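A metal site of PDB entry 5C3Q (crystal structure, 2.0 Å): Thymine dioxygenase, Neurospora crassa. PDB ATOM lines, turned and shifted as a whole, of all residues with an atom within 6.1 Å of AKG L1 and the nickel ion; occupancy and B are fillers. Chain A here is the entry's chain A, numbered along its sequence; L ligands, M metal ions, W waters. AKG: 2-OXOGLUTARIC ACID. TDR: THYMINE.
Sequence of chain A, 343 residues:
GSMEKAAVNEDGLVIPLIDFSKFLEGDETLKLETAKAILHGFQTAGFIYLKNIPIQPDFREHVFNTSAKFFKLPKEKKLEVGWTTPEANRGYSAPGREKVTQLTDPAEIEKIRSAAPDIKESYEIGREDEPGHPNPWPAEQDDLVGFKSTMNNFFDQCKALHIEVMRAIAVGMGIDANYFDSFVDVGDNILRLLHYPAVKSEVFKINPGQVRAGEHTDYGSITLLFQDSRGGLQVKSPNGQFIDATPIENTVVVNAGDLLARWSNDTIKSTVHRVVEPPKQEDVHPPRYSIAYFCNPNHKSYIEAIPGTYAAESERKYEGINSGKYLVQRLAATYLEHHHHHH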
ATOM      1  N   LYS A 120       8.639  25.330  -9.575  1.00  0.00           N
ATOM      2  CA  LYS A 120       9.552  25.843  -8.556  1.00  0.00           C
ATOM      3  C   LYS A 120      10.574  26.792  -9.165  1.00  0.00           C
ATOM      4  O   LYS A 120      10.776  26.785 -10.376  1.00  0.00           O
ATOM      5  CB  LYS A 120      10.274  24.677  -7.867  1.00  0.00           C
ATOM      6  CG  LYS A 120      11.287  23.932  -8.749  1.00  0.00           C
ATOM      7  CD  LYS A 120      12.030  22.864  -7.977  1.00  0.00           C
ATOM      8  CE  LYS A 120      13.111  22.211  -8.842  1.00  0.00           C
ATOM      9  NZ  LYS A 120      13.952  21.266  -8.047  1.00  0.00           N
ATOM     10  N   ARG A 192      20.769  26.494  -1.167  1.00  0.00           N
ATOM     11  CA  ARG A 192      19.702  26.558  -2.169  1.00  0.00           C
ATOM     12  C   ARG A 192      18.428  27.157  -1.575  1.00  0.00           C
ATOM     13  O   ARG A 192      17.747  26.527  -0.760  1.00  0.00           O
ATOM     14  CB  ARG A 192      19.408  25.169  -2.737  1.00  0.00           C
ATOM     15  CG  ARG A 192      18.324  25.160  -3.803  1.00  0.00           C
ATOM     16  CD  ARG A 192      17.962  23.752  -4.241  1.00  0.00           C
ATOM     17  NE  ARG A 192      18.605  23.378  -5.489  1.00  0.00           N
ATOM     18  CZ  ARG A 192      18.391  22.240  -6.147  1.00  0.00           C
ATOM     19  NH1 ARG A 192      17.548  21.324  -5.667  1.00  0.00           N
ATOM     20  NH2 ARG A 192      19.035  22.007  -7.285  1.00  0.00           N
ATOM     21  N   LEU A 194      14.651  28.100  -2.147  1.00  0.00           N
ATOM     22  CA  LEU A 194      13.579  27.553  -2.976  1.00  0.00           C
ATOM     23  C   LEU A 194      12.275  28.311  -2.780  1.00  0.00           C
ATOM     24  O   LEU A 194      11.883  28.621  -1.652  1.00  0.00           O
ATOM     25  CB  LEU A 194      13.352  26.077  -2.656  1.00  0.00           C
ATOM     26  CG  LEU A 194      14.414  25.119  -3.195  1.00  0.00           C
ATOM     27  CD1 LEU A 194      14.487  23.849  -2.346  1.00  0.00           C
ATOM     28  CD2 LEU A 194      14.123  24.780  -4.649  1.00  0.00           C
ATOM     29  N   TYR A 196       8.322  27.810  -4.274  1.00  0.00           N
ATOM     30  CA  TYR A 196       7.340  27.077  -5.053  1.00  0.00           C
ATOM     31  C   TYR A 196       6.115  27.980  -5.178  1.00  0.00           C
ATOM     32  O   TYR A 196       5.376  28.148  -4.214  1.00  0.00           O
ATOM     33  CB  TYR A 196       6.976  25.767  -4.364  1.00  0.00           C
ATOM     34  CG  TYR A 196       8.138  24.841  -4.101  1.00  0.00           C
ATOM     35  CD1 TYR A 196       8.890  24.928  -2.933  1.00  0.00           C
ATOM     36  CD2 TYR A 196       8.498  23.855  -5.027  1.00  0.00           C
ATOM     37  CE1 TYR A 196       9.968  24.082  -2.690  1.00  0.00           C
ATOM     38  CE2 TYR A 196       9.562  23.000  -4.791  1.00  0.00           C
ATOM     39  CZ  TYR A 196      10.295  23.120  -3.624  1.00  0.00           C
ATOM     40  OH  TYR A 196      11.341  22.259  -3.404  1.00  0.00           O
ATOM     41  N   ALA A 213       8.592  19.298  -6.687  1.00  0.00           N
ATOM     42  CA  ALA A 213       9.977  18.853  -6.855  1.00  0.00           C
ATOM     43  C   ALA A 213      10.013  17.345  -7.136  1.00  0.00           C
ATOM     44  O   ALA A 213       9.517  16.558  -6.340  1.00  0.00           O
ATOM     45  CB  ALA A 213      10.810  19.167  -5.629  1.00  0.00           C
ATOM     46  N   HIS A 216      14.069  12.276  -6.033  1.00  0.00           N
ATOM     47  CA  HIS A 216      15.509  12.233  -6.187  1.00  0.00           C
ATOM     48  C   HIS A 216      16.178  11.846  -4.873  1.00  0.00           C
ATOM     49  O   HIS A 216      15.518  11.793  -3.828  1.00  0.00           O
ATOM     50  CB  HIS A 216      16.021  13.605  -6.601  1.00  0.00           C
ATOM     51  CG  HIS A 216      15.782  14.650  -5.567  1.00  0.00           C
ATOM     52  ND1 HIS A 216      14.531  15.162  -5.308  1.00  0.00           N
ATOM     53  CD2 HIS A 216      16.621  15.243  -4.682  1.00  0.00           C
ATOM     54  CE1 HIS A 216      14.611  16.045  -4.324  1.00  0.00           C
ATOM     55  NE2 HIS A 216      15.859  16.108  -3.927  1.00  0.00           N
ATOM     56  N   THR A 217      17.473  11.573  -4.940  1.00  0.00           N
ATOM     57  CA  THR A 217      18.325  11.524  -3.770  1.00  0.00           C
ATOM     58  C   THR A 217      19.257  12.726  -3.812  1.00  0.00           C
ATOM     59  O   THR A 217      19.615  13.214  -4.901  1.00  0.00           O
ATOM     60  CB  THR A 217      19.158  10.227  -3.714  1.00  0.00           C
ATOM     61  OG1 THR A 217      19.921  10.085  -4.914  1.00  0.00           O
ATOM     62  CG2 THR A 217      18.262   9.008  -3.542  1.00  0.00           C
ATOM     63  N   ASP A 218      19.646  13.226  -2.636  1.00  0.00           N
ATOM     64  CA  ASP A 218      20.640  14.285  -2.548  1.00  0.00           C
ATOM     65  C   ASP A 218      22.031  13.692  -2.748  1.00  0.00           C
ATOM     66  O   ASP A 218      22.232  12.498  -2.541  1.00  0.00           O
ATOM     67  CB  ASP A 218      20.554  15.012  -1.195  1.00  0.00           C
ATOM     68  CG  ASP A 218      19.289  15.860  -1.062  1.00  0.00           C
ATOM     69  OD1 ASP A 218      18.510  16.004  -2.022  1.00  0.00           O
ATOM     70  OD2 ASP A 218      19.074  16.408   0.047  1.00  0.00           O
ATOM     71  N   THR A 223      22.071  17.101   4.035  1.00  0.00           N
ATOM     72  CA  THR A 223      21.333  18.274   3.637  1.00  0.00           C
ATOM     73  C   THR A 223      20.577  18.774   4.851  1.00  0.00           C
ATOM     74  O   THR A 223      19.962  17.989   5.572  1.00  0.00           O
ATOM     75  CB  THR A 223      20.340  17.979   2.487  1.00  0.00           C
ATOM     76  OG1 THR A 223      21.062  17.502   1.350  1.00  0.00           O
ATOM     77  CG2 THR A 223      19.563  19.235   2.093  1.00  0.00           C
ATOM     78  N   LEU A 225      17.497  20.859   5.650  1.00  0.00           N
ATOM     79  CA  LEU A 225      16.298  21.357   4.989  1.00  0.00           C
ATOM     80  C   LEU A 225      15.408  22.114   5.961  1.00  0.00           C
ATOM     81  O   LEU A 225      14.858  21.529   6.898  1.00  0.00           O
ATOM     82  CB  LEU A 225      15.512  20.214   4.348  1.00  0.00           C
ATOM     83  CG  LEU A 225      14.280  20.710   3.573  1.00  0.00           C
ATOM     84  CD1 LEU A 225      14.671  21.331   2.246  1.00  0.00           C
ATOM     85  CD2 LEU A 225      13.294  19.582   3.358  1.00  0.00           C
ATOM     86  N   PHE A 226      15.287  23.415   5.734  1.00  0.00           N
ATOM     87  CA  PHE A 226      14.410  24.271   6.504  1.00  0.00           C
ATOM     88  C   PHE A 226      13.144  24.479   5.669  1.00  0.00           C
ATOM     89  O   PHE A 226      13.209  24.997   4.556  1.00  0.00           O
ATOM     90  CB  PHE A 226      15.092  25.621   6.757  1.00  0.00           C
ATOM     91  CG  PHE A 226      16.439  25.517   7.436  1.00  0.00           C
ATOM     92  CD1 PHE A 226      17.594  25.305   6.686  1.00  0.00           C
ATOM     93  CD2 PHE A 226      16.555  25.636   8.805  1.00  0.00           C
ATOM     94  CE1 PHE A 226      18.831  25.216   7.289  1.00  0.00           C
ATOM     95  CE2 PHE A 226      17.793  25.539   9.429  1.00  0.00           C
ATOM     96  CZ  PHE A 226      18.929  25.330   8.667  1.00  0.00           C
ATOM     97  N   GLN A 227      11.999  24.030   6.189  1.00  0.00           N
ATOM     98  CA  GLN A 227      10.733  24.184   5.469  1.00  0.00           C
ATOM     99  C   GLN A 227       9.758  25.036   6.270  1.00  0.00           C
ATOM    100  O   GLN A 227       9.808  25.051   7.507  1.00  0.00           O
ATOM    101  CB  GLN A 227      10.121  22.819   5.120  1.00  0.00           C
ATOM    102  CG  GLN A 227       9.688  21.953   6.300  1.00  0.00           C
ATOM    103  CD  GLN A 227       9.031  20.641   5.863  1.00  0.00           C
ATOM    104  OE1 GLN A 227       8.501  20.535   4.765  1.00  0.00           O
ATOM    105  NE2 GLN A 227       9.057  19.647   6.741  1.00  0.00           N
ATOM    106  N   LEU A 233       6.500  17.907   1.347  1.00  0.00           N
ATOM    107  CA  LEU A 233       7.688  17.057   1.355  1.00  0.00           C
ATOM    108  C   LEU A 233       7.316  15.630   1.728  1.00  0.00           C
ATOM    109  O   LEU A 233       6.585  15.402   2.692  1.00  0.00           O
ATOM    110  CB  LEU A 233       8.742  17.593   2.324  1.00  0.00           C
ATOM    111  CG  LEU A 233       9.997  16.732   2.507  1.00  0.00           C
ATOM    112  CD1 LEU A 233      10.813  16.668   1.220  1.00  0.00           C
ATOM    113  CD2 LEU A 233      10.849  17.273   3.645  1.00  0.00           C
ATOM    114  N   ASN A 255      18.905  15.078   6.191  1.00  0.00           N
ATOM    115  CA  ASN A 255      19.025  13.796   5.518  1.00  0.00           C
ATOM    116  C   ASN A 255      20.417  13.572   4.963  1.00  0.00           C
ATOM    117  O   ASN A 255      21.081  14.509   4.522  1.00  0.00           O
ATOM    118  CB  ASN A 255      17.981  13.676   4.412  1.00  0.00           C
ATOM    119  CG  ASN A 255      18.204  14.658   3.275  1.00  0.00           C
ATOM    120  OD1 ASN A 255      17.892  15.838   3.406  1.00  0.00           O
ATOM    121  ND2 ASN A 255      18.729  14.178   2.155  1.00  0.00           N
ATOM    122  N   HIS A 273      13.222  11.261  -1.889  1.00  0.00           N
ATOM    123  CA  HIS A 273      12.221  12.202  -1.441  1.00  0.00           C
ATOM    124  C   HIS A 273      11.775  13.117  -2.575  1.00  0.00           C
ATOM    125  O   HIS A 273      12.421  13.190  -3.617  1.00  0.00           O
ATOM    126  CB  HIS A 273      12.739  13.022  -0.251  1.00  0.00           C
ATOM    127  CG  HIS A 273      14.071  13.662  -0.497  1.00  0.00           C
ATOM    128  ND1 HIS A 273      15.237  12.934  -0.614  1.00  0.00           N
ATOM    129  CD2 HIS A 273      14.409  14.963  -0.653  1.00  0.00           C
ATOM    130  CE1 HIS A 273      16.243  13.766  -0.831  1.00  0.00           C
ATOM    131  NE2 HIS A 273      15.767  14.993  -0.866  1.00  0.00           N
ATOM    132  N   ARG A 274      10.654  13.802  -2.365  1.00  0.00           N
ATOM    133  CA  ARG A 274      10.053  14.648  -3.385  1.00  0.00           C
ATOM    134  C   ARG A 274       9.178  15.698  -2.705  1.00  0.00           C
ATOM    135  O   ARG A 274       8.979  15.650  -1.490  1.00  0.00           O
ATOM    136  CB  ARG A 274       9.196  13.806  -4.349  1.00  0.00           C
ATOM    137  CG  ARG A 274       7.910  13.276  -3.739  1.00  0.00           C
ATOM    138  CD  ARG A 274       7.218  12.271  -4.651  1.00  0.00           C
ATOM    139  NE  ARG A 274       5.939  11.845  -4.093  1.00  0.00           N
ATOM    140  CZ  ARG A 274       5.042  11.104  -4.731  1.00  0.00           C
ATOM    141  NH1 ARG A 274       5.266  10.681  -5.970  1.00  0.00           N
ATOM    142  NH2 ARG A 274       3.898  10.784  -4.128  1.00  0.00           N
ATOM    143  N   VAL A 275       8.674  16.641  -3.491  1.00  0.00           N
ATOM    144  CA  VAL A 275       7.678  17.590  -3.006  1.00  0.00           C
ATOM    145  C   VAL A 275       6.473  17.558  -3.938  1.00  0.00           C
ATOM    146  O   VAL A 275       6.616  17.763  -5.148  1.00  0.00           O
ATOM    147  CB  VAL A 275       8.217  19.024  -2.906  1.00  0.00           C
ATOM    148  CG1 VAL A 275       7.191  19.938  -2.246  1.00  0.00           C
ATOM    149  CG2 VAL A 275       9.517  19.064  -2.099  1.00  0.00           C
ATOM    150  N   ARG A 288       5.011  28.150  -1.334  1.00  0.00           N
ATOM    151  CA  ARG A 288       5.812  27.407  -0.370  1.00  0.00           C
ATOM    152  C   ARG A 288       7.281  27.840  -0.480  1.00  0.00           C
ATOM    153  O   ARG A 288       7.840  27.930  -1.574  1.00  0.00           O
ATOM    154  CB  ARG A 288       5.688  25.899  -0.607  1.00  0.00           C
ATOM    155  CG  ARG A 288       6.625  25.036   0.234  1.00  0.00           C
ATOM    156  CD  ARG A 288       6.254  23.568   0.181  1.00  0.00           C
ATOM    157  NE  ARG A 288       7.012  22.768   1.149  1.00  0.00           N
ATOM    158  CZ  ARG A 288       8.246  22.302   0.965  1.00  0.00           C
ATOM    159  NH1 ARG A 288       8.913  22.547  -0.162  1.00  0.00           N
ATOM    160  NH2 ARG A 288       8.821  21.586   1.924  1.00  0.00           N
ATOM    161  N   SER A 290      11.177  26.968   0.993  1.00  0.00           N
ATOM    162  CA  SER A 290      12.105  26.149   1.746  1.00  0.00           C
ATOM    163  C   SER A 290      13.525  26.567   1.418  1.00  0.00           C
ATOM    164  O   SER A 290      13.772  27.305   0.446  1.00  0.00           O
ATOM    165  CB  SER A 290      11.894  24.656   1.433  1.00  0.00           C
ATOM    166  OG  SER A 290      12.194  24.362   0.085  1.00  0.00           O
ATOM    167  N   ILE A 291      14.448  26.121   2.258  1.00  0.00           N
ATOM    168  CA  ILE A 291      15.861  26.360   2.063  1.00  0.00           C
ATOM    169  C   ILE A 291      16.573  25.030   2.251  1.00  0.00           C
ATOM    170  O   ILE A 291      16.503  24.416   3.333  1.00  0.00           O
ATOM    171  CB  ILE A 291      16.410  27.407   3.051  1.00  0.00           C
ATOM    172  CG1 ILE A 291      15.619  28.711   2.924  1.00  0.00           C
ATOM    173  CG2 ILE A 291      17.898  27.638   2.798  1.00  0.00           C
ATOM    174  CD1 ILE A 291      16.014  29.793   3.917  1.00  0.00           C
ATOM    175  N   ALA A 292      17.243  24.563   1.196  1.00  0.00           N
ATOM    176  CA  ALA A 292      18.072  23.367   1.266  1.00  0.00           C
ATOM    177  C   ALA A 292      19.533  23.775   1.310  1.00  0.00           C
ATOM    178  O   ALA A 292      20.051  24.365   0.358  1.00  0.00           O
ATOM    179  CB  ALA A 292      17.807  22.472   0.071  1.00  0.00           C
ATOM    180  N   PHE A 294      22.870  22.178   1.080  1.00  0.00           N
ATOM    181  CA  PHE A 294      23.567  20.956   0.697  1.00  0.00           C
ATOM    182  C   PHE A 294      24.969  20.981   1.269  1.00  0.00           C
ATOM    183  O   PHE A 294      25.782  21.840   0.907  1.00  0.00           O
ATOM    184  CB  PHE A 294      23.641  20.826  -0.823  1.00  0.00           C
ATOM    185  CG  PHE A 294      22.305  20.780  -1.501  1.00  0.00           C
ATOM    186  CD1 PHE A 294      21.403  19.770  -1.202  1.00  0.00           C
ATOM    187  CD2 PHE A 294      21.957  21.726  -2.451  1.00  0.00           C
ATOM    188  CE1 PHE A 294      20.171  19.711  -1.837  1.00  0.00           C
ATOM    189  CE2 PHE A 294      20.725  21.676  -3.082  1.00  0.00           C
ATOM    190  CZ  PHE A 294      19.828  20.663  -2.774  1.00  0.00           C
HETATM  191  C1  AKG L   1      16.007  19.660  -2.756  1.00  0.00           C
HETATM  192  O1  AKG L   1      16.894  18.795  -2.990  1.00  0.00           O
HETATM  193  O2  AKG L   1      16.098  20.834  -3.165  1.00  0.00           O
HETATM  194  C2  AKG L   1      14.818  19.265  -1.984  1.00  0.00           C
HETATM  195  O5  AKG L   1      14.625  18.086  -1.712  1.00  0.00           O
HETATM  196  C3  AKG L   1      13.833  20.334  -1.536  1.00  0.00           C
HETATM  197  C4  AKG L   1      12.763  19.737  -0.616  1.00  0.00           C
HETATM  198  C5  AKG L   1      11.826  20.804  -0.099  1.00  0.00           C
HETATM  199  O3  AKG L   1      11.237  20.577   0.989  1.00  0.00           O
HETATM  200  O4  AKG L   1      11.651  21.865  -0.744  1.00  0.00           O
HETATM  201  N1  TDR L   2      22.212  20.307  -6.064  1.00  0.00           N
HETATM  202  C2  TDR L   2      23.339  20.048  -5.191  1.00  0.00           C
HETATM  203  O2  TDR L   2      24.309  20.770  -5.233  1.00  0.00           O
HETATM  204  N3  TDR L   2      23.286  18.930  -4.275  1.00  0.00           N
HETATM  205  C4  TDR L   2      22.147  18.078  -4.217  1.00  0.00           C
HETATM  206  O4  TDR L   2      22.145  17.151  -3.432  1.00  0.00           O
HETATM  207  C5  TDR L   2      21.002  18.332  -5.106  1.00  0.00           C
HETATM  208  CM5 TDR L   2      19.782  17.466  -5.103  1.00  0.00           C
HETATM  209  C6  TDR L   2      21.059  19.464  -6.031  1.00  0.00           C
HETATM  210 NI    NI M   1      16.461  16.841  -1.932  1.00  0.00          NI
HETATM  211  O   HOH W   1      16.962  17.785   0.004  1.00  0.00           O
HETATM  212  O   HOH W   2      13.794  21.318  -5.052  1.00  0.00           O
HETATM  213  O   HOH W   3      16.483  18.548  -6.001  1.00  0.00           O
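Water W2 lies within hydrogen-bond range of the side-chain amino group (NZ) of Lys 120 (3.0 Å), an oxygen (O2) of AKG L1 (3.0 Å) and the side-chain hydroxyl (OH) of Tyr 196 (3.1 Å).
NE2 of His 216 is bound to the nickel ion.
Water W1 is bound to the nickel ion.
OD1 of Asp 218 is bound to the nickel ion.
The nickel ion is bound by O5 of AKG L1, 2.2 Å away.
NE2 of His 273 is bound to the nickel ion.
The nickel ion is bound by O1 of AKG L1 (2.3 Å).
Three residues have an atom within 4 Å of the nickel ion: His 216, Asp 218 and His 273.
The nearest printed residue that does not touch the nickel ion is Phe 294 (4.7 Å).
The guanidinium group (NH1) of Arg 192 is in salt-bridge range of an oxygen (O2) of AKG L1 (2.9 Å).
An oxygen (O4) of AKG L1 lies within hydrogen-bond range of the side-chain hydroxyl (OG) of Ser 290 (2.7 Å).
An oxygen (O3) of AKG L1 lies within salt-bridge range of the guanidinium group of Arg 288 (2.8 Å).
The side-chain hydroxyl (OH) of Tyr 196 sits at hydrogen-bond distance from an oxygen (O4) of AKG L1, 2.7 Å away.
Merely in contact with AKG L1: Leu 194, Leu 225, Leu 233, Val 275 and Phe 294.
Hydrophobic or aromatic side chains within 4 Å of AKG L1: Leu 194, Tyr 196, His 216, Leu 225, Leu 233, His 273, Val 275 and Phe 294.
12 residues have an atom within 4 Å of AKG L1: Arg 192, Leu 194, Tyr 196, His 216, Asp 218, Leu 225, Leu 233, His 273, Val 275, Arg 288, Ser 290 and Phe 294.
The nearest printed residue that does not touch AKG L1 is Ala 292 (4.01 Å).
The side-chain amide oxygen (OE1) of Gln 227 is in hydrogen-bond range of the guanidinium group (NH2) of Arg 288.
O of Arg 288 sits at hydrogen-bond distance from N of Tyr 196, 2.7 Å away.
N of Arg 192 lies within hydrogen-bond range of O of Ala 292, at 2.7 Å.
The backbone carbonyl oxygen (O) of Val 275 sits at hydrogen-bond distance from the backbone NH (N) of Ala 213 (2.9 Å).
O of Ser 290 lies within hydrogen-bond range of N of Leu 194.
The side-chain carboxylate of Asp 218 is in hydrogen-bond range of the side-chain hydroxyl of Thr 223 (2.6 Å).
OD2 of Asp 218 sits at hydrogen-bond distance from ND2 of Asn 255 (3.1 Å).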
